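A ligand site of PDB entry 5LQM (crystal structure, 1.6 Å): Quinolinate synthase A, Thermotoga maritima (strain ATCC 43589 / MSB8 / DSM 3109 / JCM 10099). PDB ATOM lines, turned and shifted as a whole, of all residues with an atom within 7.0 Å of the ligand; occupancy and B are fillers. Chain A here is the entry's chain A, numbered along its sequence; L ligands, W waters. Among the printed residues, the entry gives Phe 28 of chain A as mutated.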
ATOM      1  N   HIS A  26     -21.480 -10.604 -24.762  1.00  0.00           N
ATOM      2  CA  HIS A  26     -21.872 -11.696 -23.914  1.00  0.00           C
ATOM      3  C   HIS A  26     -22.675 -11.198 -22.704  1.00  0.00           C
ATOM      4  O   HIS A  26     -22.426 -10.093 -22.198  1.00  0.00           O
ATOM      5  CB  HIS A  26     -20.632 -12.515 -23.485  1.00  0.00           C
ATOM      6  CG  HIS A  26     -20.990 -13.788 -22.787  1.00  0.00           C
ATOM      7  ND1 HIS A  26     -21.143 -13.861 -21.420  1.00  0.00           N
ATOM      8  CD2 HIS A  26     -21.376 -14.980 -23.270  1.00  0.00           C
ATOM      9  CE1 HIS A  26     -21.566 -15.064 -21.097  1.00  0.00           C
ATOM     10  NE2 HIS A  26     -21.710 -15.761 -22.199  1.00  0.00           N
ATOM     11  N   PHE A  28     -22.260 -11.709 -19.639  1.00  0.00           N
ATOM     12  CA  PHE A  28     -21.495 -11.418 -18.435  1.00  0.00           C
ATOM     13  C   PHE A  28     -20.776 -10.086 -18.542  1.00  0.00           C
ATOM     14  O   PHE A  28     -20.046  -9.712 -17.631  1.00  0.00           O
ATOM     15  CB  PHE A  28     -20.456 -12.506 -18.117  1.00  0.00           C
ATOM     16  CG  PHE A  28     -21.030 -13.861 -17.850  1.00  0.00           C
ATOM     17  CD1 PHE A  28     -22.377 -14.055 -17.551  1.00  0.00           C
ATOM     18  CD2 PHE A  28     -20.182 -14.977 -17.845  1.00  0.00           C
ATOM     19  CE1 PHE A  28     -22.871 -15.312 -17.276  1.00  0.00           C
ATOM     20  CE2 PHE A  28     -20.668 -16.255 -17.572  1.00  0.00           C
ATOM     21  CZ  PHE A  28     -22.031 -16.410 -17.282  1.00  0.00           C
ATOM     22  N   VAL A  63     -14.950 -12.661 -24.134  1.00  0.00           N
ATOM     23  CA  VAL A  63     -13.572 -13.209 -24.003  1.00  0.00           C
ATOM     24  C   VAL A  63     -13.058 -13.735 -25.329  1.00  0.00           C
ATOM     25  O   VAL A  63     -13.829 -13.959 -26.248  1.00  0.00           O
ATOM     26  CB  VAL A  63     -13.406 -14.241 -22.872  1.00  0.00           C
ATOM     27  CG1 VAL A  63     -13.655 -13.563 -21.522  1.00  0.00           C
ATOM     28  CG2 VAL A  63     -14.305 -15.445 -23.078  1.00  0.00           C
ATOM     29  N   MET A  66     -14.410 -16.545 -27.751  1.00  0.00           N
ATOM     30  CA  MET A  66     -15.670 -16.119 -28.372  1.00  0.00           C
ATOM     31  C   MET A  66     -15.406 -15.164 -29.557  1.00  0.00           C
ATOM     32  O   MET A  66     -15.902 -15.344 -30.677  1.00  0.00           O
ATOM     33  CB  MET A  66     -16.565 -15.397 -27.345  1.00  0.00           C
ATOM     34  CG  MET A  66     -16.944 -16.140 -26.046  1.00  0.00           C
ATOM     35  SD  MET A  66     -17.878 -15.085 -24.880  1.00  0.00           S
ATOM     36  CE  MET A  66     -18.217 -16.353 -23.676  1.00  0.00           C
ATOM     37  N   THR A  87      -9.751 -13.309 -21.487  1.00  0.00           N
ATOM     38  CA  THR A  87      -9.596 -14.720 -21.839  1.00  0.00           C
ATOM     39  C   THR A  87     -10.348 -15.590 -20.824  1.00  0.00           C
ATOM     40  O   THR A  87     -10.828 -15.100 -19.827  1.00  0.00           O
ATOM     41  CB  THR A  87      -8.096 -15.107 -21.944  1.00  0.00           C
ATOM     42  OG1 THR A  87      -7.985 -16.390 -22.592  1.00  0.00           O
ATOM     43  CG2 THR A  87      -7.417 -15.149 -20.614  1.00  0.00           C
ATOM     44  N   CYS A  88     -10.414 -16.884 -21.083  1.00  0.00           N
ATOM     45  CA  CYS A  88     -11.040 -17.816 -20.136  1.00  0.00           C
ATOM     46  C   CYS A  88      -9.942 -18.745 -19.634  1.00  0.00           C
ATOM     47  O   CYS A  88      -9.415 -19.517 -20.410  1.00  0.00           O
ATOM     48  CB  CYS A  88     -12.157 -18.580 -20.825  1.00  0.00           C
ATOM     49  SG  CYS A  88     -12.858 -19.880 -19.781  1.00  0.00           S
ATOM     50  N   PRO A  89      -9.543 -18.624 -18.363  1.00  0.00           N
ATOM     51  CA  PRO A  89      -8.449 -19.475 -17.849  1.00  0.00           C
ATOM     52  C   PRO A  89      -8.702 -20.975 -17.974  1.00  0.00           C
ATOM     53  O   PRO A  89      -7.761 -21.712 -18.173  1.00  0.00           O
ATOM     54  CB  PRO A  89      -8.344 -19.044 -16.377  1.00  0.00           C
ATOM     55  CG  PRO A  89      -8.806 -17.636 -16.385  1.00  0.00           C
ATOM     56  CD  PRO A  89      -9.937 -17.608 -17.355  1.00  0.00           C
ATOM     57  N   MET A  90      -9.957 -21.398 -17.857  1.00  0.00           N
ATOM     58  CA  MET A  90     -10.283 -22.817 -18.008  1.00  0.00           C
ATOM     59  C   MET A  90      -9.986 -23.329 -19.407  1.00  0.00           C
ATOM     60  O   MET A  90      -9.358 -24.370 -19.576  1.00  0.00           O
ATOM     61  CB  MET A  90     -11.751 -23.053 -17.735  1.00  0.00           C
ATOM     62  CG  MET A  90     -12.168 -24.495 -17.947  1.00  0.00           C
ATOM     63  SD  MET A  90     -13.905 -24.678 -17.642  1.00  0.00           S
ATOM     64  CE  MET A  90     -14.620 -23.919 -19.111  1.00  0.00           C
ATOM     65  N   ALA A  91     -10.449 -22.567 -20.380  1.00  0.00           N
ATOM     66  CA  ALA A  91     -10.214 -22.866 -21.779  1.00  0.00           C
ATOM     67  C   ALA A  91      -8.725 -23.046 -22.025  1.00  0.00           C
ATOM     68  O   ALA A  91      -8.320 -23.952 -22.724  1.00  0.00           O
ATOM     69  CB  ALA A  91     -10.784 -21.752 -22.634  1.00  0.00           C
ATOM     70  N   TYR A 114     -15.781 -27.969 -25.769  1.00  0.00           N
ATOM     71  CA  TYR A 114     -16.602 -26.879 -25.333  1.00  0.00           C
ATOM     72  C   TYR A 114     -16.112 -25.645 -26.076  1.00  0.00           C
ATOM     73  O   TYR A 114     -14.926 -25.518 -26.346  1.00  0.00           O
ATOM     74  CB  TYR A 114     -16.372 -26.681 -23.832  1.00  0.00           C
ATOM     75  CG  TYR A 114     -17.362 -25.818 -23.077  1.00  0.00           C
ATOM     76  CD1 TYR A 114     -18.635 -25.532 -23.585  1.00  0.00           C
ATOM     77  CD2 TYR A 114     -17.041 -25.355 -21.819  1.00  0.00           C
ATOM     78  CE1 TYR A 114     -19.527 -24.761 -22.853  1.00  0.00           C
ATOM     79  CE2 TYR A 114     -17.938 -24.623 -21.055  1.00  0.00           C
ATOM     80  CZ  TYR A 114     -19.180 -24.328 -21.590  1.00  0.00           C
ATOM     81  OH  TYR A 114     -20.103 -23.597 -20.853  1.00  0.00           O
ATOM     82  N   ASN A 116     -15.464 -22.834 -24.929  1.00  0.00           N
ATOM     83  CA  ASN A 116     -14.383 -22.308 -24.124  1.00  0.00           C
ATOM     84  C   ASN A 116     -13.125 -23.201 -24.349  1.00  0.00           C
ATOM     85  O   ASN A 116     -12.808 -24.042 -23.499  1.00  0.00           O
ATOM     86  CB  ASN A 116     -14.744 -22.283 -22.603  1.00  0.00           C
ATOM     87  CG  ASN A 116     -16.165 -21.769 -22.300  1.00  0.00           C
ATOM     88  OD1 ASN A 116     -17.122 -22.093 -23.000  1.00  0.00           O
ATOM     89  ND2 ASN A 116     -16.313 -21.008 -21.225  1.00  0.00           N
ATOM     90  N   ASP A 151     -14.099 -28.535 -19.627  1.00  0.00           N
ATOM     91  CA  ASP A 151     -14.850 -28.369 -18.368  1.00  0.00           C
ATOM     92  C   ASP A 151     -15.381 -29.720 -17.893  1.00  0.00           C
ATOM     93  O   ASP A 151     -16.256 -30.309 -18.540  1.00  0.00           O
ATOM     94  CB  ASP A 151     -15.986 -27.367 -18.542  1.00  0.00           C
ATOM     95  CG  ASP A 151     -16.653 -26.973 -17.217  1.00  0.00           C
ATOM     96  OD1 ASP A 151     -17.487 -27.716 -16.712  1.00  0.00           O
ATOM     97  OD2 ASP A 151     -16.373 -25.879 -16.697  1.00  0.00           O
ATOM     98  N   HIS A 174     -12.182 -26.754 -14.782  1.00  0.00           N
ATOM     99  CA  HIS A 174     -13.387 -26.211 -14.213  1.00  0.00           C
ATOM    100  C   HIS A 174     -13.331 -24.710 -14.262  1.00  0.00           C
ATOM    101  O   HIS A 174     -12.252 -24.100 -14.429  1.00  0.00           O
ATOM    102  CB  HIS A 174     -13.551 -26.664 -12.751  1.00  0.00           C
ATOM    103  CG  HIS A 174     -12.538 -26.070 -11.818  1.00  0.00           C
ATOM    104  ND1 HIS A 174     -11.241 -26.523 -11.739  1.00  0.00           N
ATOM    105  CD2 HIS A 174     -12.635 -25.021 -10.965  1.00  0.00           C
ATOM    106  CE1 HIS A 174     -10.576 -25.785 -10.862  1.00  0.00           C
ATOM    107  NE2 HIS A 174     -11.399 -24.863 -10.388  1.00  0.00           N
ATOM    108  N   CYS A 175     -14.500 -24.109 -14.108  1.00  0.00           N
ATOM    109  CA  CYS A 175     -14.648 -22.691 -13.991  1.00  0.00           C
ATOM    110  C   CYS A 175     -14.743 -22.298 -12.516  1.00  0.00           C
ATOM    111  O   CYS A 175     -15.765 -22.612 -11.889  1.00  0.00           O
ATOM    112  CB  CYS A 175     -15.921 -22.260 -14.678  1.00  0.00           C
ATOM    113  SG  CYS A 175     -16.272 -20.501 -14.418  1.00  0.00           S
ATOM    114  N   PRO A 176     -13.751 -21.561 -11.993  1.00  0.00           N
ATOM    115  CA  PRO A 176     -13.839 -21.059 -10.609  1.00  0.00           C
ATOM    116  C   PRO A 176     -15.106 -20.235 -10.280  1.00  0.00           C
ATOM    117  O   PRO A 176     -15.580 -20.277  -9.148  1.00  0.00           O
ATOM    118  CB  PRO A 176     -12.562 -20.224 -10.429  1.00  0.00           C
ATOM    119  CG  PRO A 176     -12.019 -19.987 -11.793  1.00  0.00           C
ATOM    120  CD  PRO A 176     -12.526 -21.081 -12.674  1.00  0.00           C
ATOM    121  N   VAL A 177     -15.637 -19.508 -11.269  1.00  0.00           N
ATOM    122  CA  VAL A 177     -16.752 -18.585 -11.048  1.00  0.00           C
ATOM    123  C   VAL A 177     -18.040 -19.311 -10.655  1.00  0.00           C
ATOM    124  O   VAL A 177     -18.797 -18.820  -9.819  1.00  0.00           O
ATOM    125  CB  VAL A 177     -16.973 -17.687 -12.305  1.00  0.00           C
ATOM    126  CG1 VAL A 177     -18.094 -16.723 -12.049  1.00  0.00           C
ATOM    127  CG2 VAL A 177     -15.694 -16.903 -12.623  1.00  0.00           C
ATOM    128  N   HIS A 178     -18.213 -20.526 -11.179  1.00  0.00           N
ATOM    129  CA  HIS A 178     -19.397 -21.355 -10.989  1.00  0.00           C
ATOM    130  C   HIS A 178     -19.278 -22.374  -9.857  1.00  0.00           C
ATOM    131  O   HIS A 178     -20.184 -23.190  -9.671  1.00  0.00           O
ATOM    132  CB  HIS A 178     -19.731 -22.051 -12.310  1.00  0.00           C
ATOM    133  CG  HIS A 178     -20.369 -21.136 -13.296  1.00  0.00           C
ATOM    134  ND1 HIS A 178     -19.645 -20.454 -14.260  1.00  0.00           N
ATOM    135  CD2 HIS A 178     -21.649 -20.744 -13.436  1.00  0.00           C
ATOM    136  CE1 HIS A 178     -20.477 -19.701 -14.968  1.00  0.00           C
ATOM    137  NE2 HIS A 178     -21.692 -19.859 -14.485  1.00  0.00           N
ATOM    138  N   HIS A 200     -26.084 -22.977 -13.690  1.00  0.00           N
ATOM    139  CA  HIS A 200     -25.364 -23.311 -14.916  1.00  0.00           C
ATOM    140  C   HIS A 200     -24.843 -24.753 -14.861  1.00  0.00           C
ATOM    141  O   HIS A 200     -24.484 -25.217 -13.788  1.00  0.00           O
ATOM    142  CB  HIS A 200     -24.171 -22.373 -15.051  1.00  0.00           C
ATOM    143  CG  HIS A 200     -23.689 -22.233 -16.446  1.00  0.00           C
ATOM    144  ND1 HIS A 200     -22.808 -23.107 -17.015  1.00  0.00           N
ATOM    145  CD2 HIS A 200     -24.037 -21.357 -17.411  1.00  0.00           C
ATOM    146  CE1 HIS A 200     -22.596 -22.753 -18.277  1.00  0.00           C
ATOM    147  NE2 HIS A 200     -23.341 -21.709 -18.536  1.00  0.00           N
ATOM    148  N   GLU A 202     -21.930 -25.707 -15.642  1.00  0.00           N
ATOM    149  CA  GLU A 202     -20.550 -25.589 -15.176  1.00  0.00           C
ATOM    150  C   GLU A 202     -20.443 -25.679 -13.651  1.00  0.00           C
ATOM    151  O   GLU A 202     -19.352 -25.811 -13.112  1.00  0.00           O
ATOM    152  CB  GLU A 202     -19.917 -24.267 -15.637  1.00  0.00           C
ATOM    153  CG  GLU A 202     -19.456 -24.238 -17.107  1.00  0.00           C
ATOM    154  CD  GLU A 202     -18.935 -22.879 -17.561  1.00  0.00           C
ATOM    155  OE1 GLU A 202     -18.510 -22.074 -16.717  1.00  0.00           O
ATOM    156  OE2 GLU A 202     -18.967 -22.579 -18.754  1.00  0.00           O
ATOM    157  N   THR A 236     -25.132 -18.325 -11.634  1.00  0.00           N
ATOM    158  CA  THR A 236     -24.138 -18.022 -12.678  1.00  0.00           C
ATOM    159  C   THR A 236     -23.446 -16.696 -12.345  1.00  0.00           C
ATOM    160  O   THR A 236     -23.618 -16.137 -11.244  1.00  0.00           O
ATOM    161  CB  THR A 236     -24.745 -18.082 -14.121  1.00  0.00           C
ATOM    162  OG1 THR A 236     -23.692 -18.102 -15.096  1.00  0.00           O
ATOM    163  CG2 THR A 236     -25.637 -16.932 -14.429  1.00  0.00           C
ATOM    164  N   GLU A 237     -22.641 -16.222 -13.296  1.00  0.00           N
ATOM    165  CA  GLU A 237     -21.908 -14.970 -13.146  1.00  0.00           C
ATOM    166  C   GLU A 237     -22.860 -13.791 -13.033  1.00  0.00           C
ATOM    167  O   GLU A 237     -23.900 -13.742 -13.703  1.00  0.00           O
ATOM    168  CB  GLU A 237     -20.947 -14.810 -14.329  1.00  0.00           C
ATOM    169  CG  GLU A 237     -19.734 -13.958 -14.025  1.00  0.00           C
ATOM    170  CD  GLU A 237     -19.907 -12.490 -14.302  1.00  0.00           C
ATOM    171  OE1 GLU A 237     -20.942 -12.063 -14.877  1.00  0.00           O
ATOM    172  OE2 GLU A 237     -18.984 -11.730 -13.931  1.00  0.00           O
ATOM    173  N   VAL A 260     -18.052 -13.266  -9.829  1.00  0.00           N
ATOM    174  CA  VAL A 260     -17.553 -12.317 -10.821  1.00  0.00           C
ATOM    175  C   VAL A 260     -16.475 -12.983 -11.650  1.00  0.00           C
ATOM    176  O   VAL A 260     -15.559 -13.584 -11.107  1.00  0.00           O
ATOM    177  CB  VAL A 260     -16.994 -11.027 -10.156  1.00  0.00           C
ATOM    178  CG1 VAL A 260     -16.426 -10.053 -11.195  1.00  0.00           C
ATOM    179  CG2 VAL A 260     -18.060 -10.362  -9.320  1.00  0.00           C
ATOM    180  N   CYS A 261     -16.582 -12.874 -12.976  1.00  0.00           N
ATOM    181  CA  CYS A 261     -15.541 -13.307 -13.892  1.00  0.00           C
ATOM    182  C   CYS A 261     -14.689 -12.050 -14.189  1.00  0.00           C
ATOM    183  O   CYS A 261     -15.154 -11.158 -14.915  1.00  0.00           O
ATOM    184  CB  CYS A 261     -16.130 -13.887 -15.189  1.00  0.00           C
ATOM    185  SG  CYS A 261     -14.814 -14.349 -16.354  1.00  0.00           S
ATOM    186  N   VAL A 262     -13.489 -11.984 -13.580  1.00  0.00           N
ATOM    187  CA  VAL A 262     -12.546 -10.871 -13.765  1.00  0.00           C
ATOM    188  C   VAL A 262     -12.307 -10.609 -15.248  1.00  0.00           C
ATOM    189  O   VAL A 262     -12.253  -9.451 -15.691  1.00  0.00           O
ATOM    190  CB  VAL A 262     -11.196 -11.174 -13.026  1.00  0.00           C
ATOM    191  CG1 VAL A 262     -10.038 -10.340 -13.542  1.00  0.00           C
ATOM    192  CG2 VAL A 262     -11.390 -10.981 -11.519  1.00  0.00           C
ATOM    193  N   ASN A 263     -12.178 -11.671 -16.027  1.00  0.00           N
ATOM    194  CA  ASN A 263     -11.912 -11.501 -17.477  1.00  0.00           C
ATOM    195  C   ASN A 263     -13.056 -10.823 -18.223  1.00  0.00           C
ATOM    196  O   ASN A 263     -12.812  -9.891 -19.030  1.00  0.00           O
ATOM    197  CB  ASN A 263     -11.464 -12.802 -18.140  1.00  0.00           C
ATOM    198  CG  ASN A 263      -9.971 -13.031 -17.968  1.00  0.00           C
ATOM    199  OD1 ASN A 263      -9.172 -12.451 -18.717  1.00  0.00           O
ATOM    200  ND2 ASN A 263      -9.585 -13.875 -17.006  1.00  0.00           N
ATOM    201  N   MET A 264     -14.289 -11.210 -17.912  1.00  0.00           N
ATOM    202  CA  MET A 264     -15.482 -10.564 -18.517  1.00  0.00           C
ATOM    203  C   MET A 264     -15.589  -9.076 -18.098  1.00  0.00           C
ATOM    204  O   MET A 264     -16.119  -8.280 -18.834  1.00  0.00           O
ATOM    205  CB  MET A 264     -16.738 -11.331 -18.132  1.00  0.00           C
ATOM    206  CG  MET A 264     -16.876 -12.653 -18.852  1.00  0.00           C
ATOM    207  SD  MET A 264     -17.374 -12.396 -20.558  1.00  0.00           S
ATOM    208  CE  MET A 264     -17.721 -14.056 -21.178  1.00  0.00           C
HETATM  209 FE1  LIG L   1     -15.796 -19.105 -16.150  1.00  0.00          FE
HETATM  210 FE2  LIG L   1     -15.265 -16.549 -17.059  1.00  0.00          FE
HETATM  211 FE3  LIG L   1     -17.054 -18.334 -18.363  1.00  0.00          FE
HETATM  212 FE4  LIG L   1     -14.363 -18.809 -18.435  1.00  0.00          FE
HETATM  213  S1  LIG L   1     -15.400 -16.981 -19.380  1.00  0.00           S
HETATM  214  S2  LIG L   1     -16.051 -20.385 -18.056  1.00  0.00           S
HETATM  215  S3  LIG L   1     -13.685 -18.100 -16.309  1.00  0.00           S
HETATM  216  S4  LIG L   1     -17.284 -17.355 -16.226  1.00  0.00           S
HETATM  217  O   HOH W   1     -11.436 -20.167 -15.574  1.00  0.00           O
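SG of Cys 175 is bound to FE1 of the ligand, 2.3 Å away.
The side-chain amide nitrogen (ND2) of Asn 116 lies close to a sulfur (S2) of the ligand (3.2 Å).
SG of Cys 261 is bound to FE2 of the ligand (2.4 Å).
SG of Cys 88 binds FE4 of the ligand, 2.3 Å away.
N of Val 177 lies close to SG of Cys 175 (3.4 Å).
ND1 of His 200 lies within hydrogen-bond range of N of Glu 202, 3.1 Å away.
The side-chain sulfur of Cys 88 sits close to the backbone NH of Met 90 (3.8 Å).
The backbone NH (N) of Phe 28 lies within hydrogen-bond range of a ring nitrogen (ND1) of His 26 (3.0 Å).
N of Met 264 lies close to SG of Cys 261.
The side-chain carboxylate (OE2) of Glu 202 lies within hydrogen-bond range of the side-chain hydroxyl (OH) of Tyr 114, 2.6 Å away.
OE2 of Glu 237 is in hydrogen-bond range of N of Cys 261 (2.8 Å).
ND1 of His 178 lies close to SG of Cys 175.
Water W1 bridges N of Met 90 and S3 of the ligand.
The side-chain carboxylate (OE1) of Glu 202 sits close to a sulfur (S2) of the ligand (3.3 Å).
Phe 28 touches the ligand.
CD of Pro 89 touches S3 of the ligand, at 3.9 Å.
Met 90 touches the ligand.
CB of Val 177 touches S4 of the ligand, at 3.9 Å.
Within 4 Å of the ligand: Phe 28, Cys 88, Pro 89, Met 90, Asn 116, Cys 175, Val 177, Glu 202 and Cys 261.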
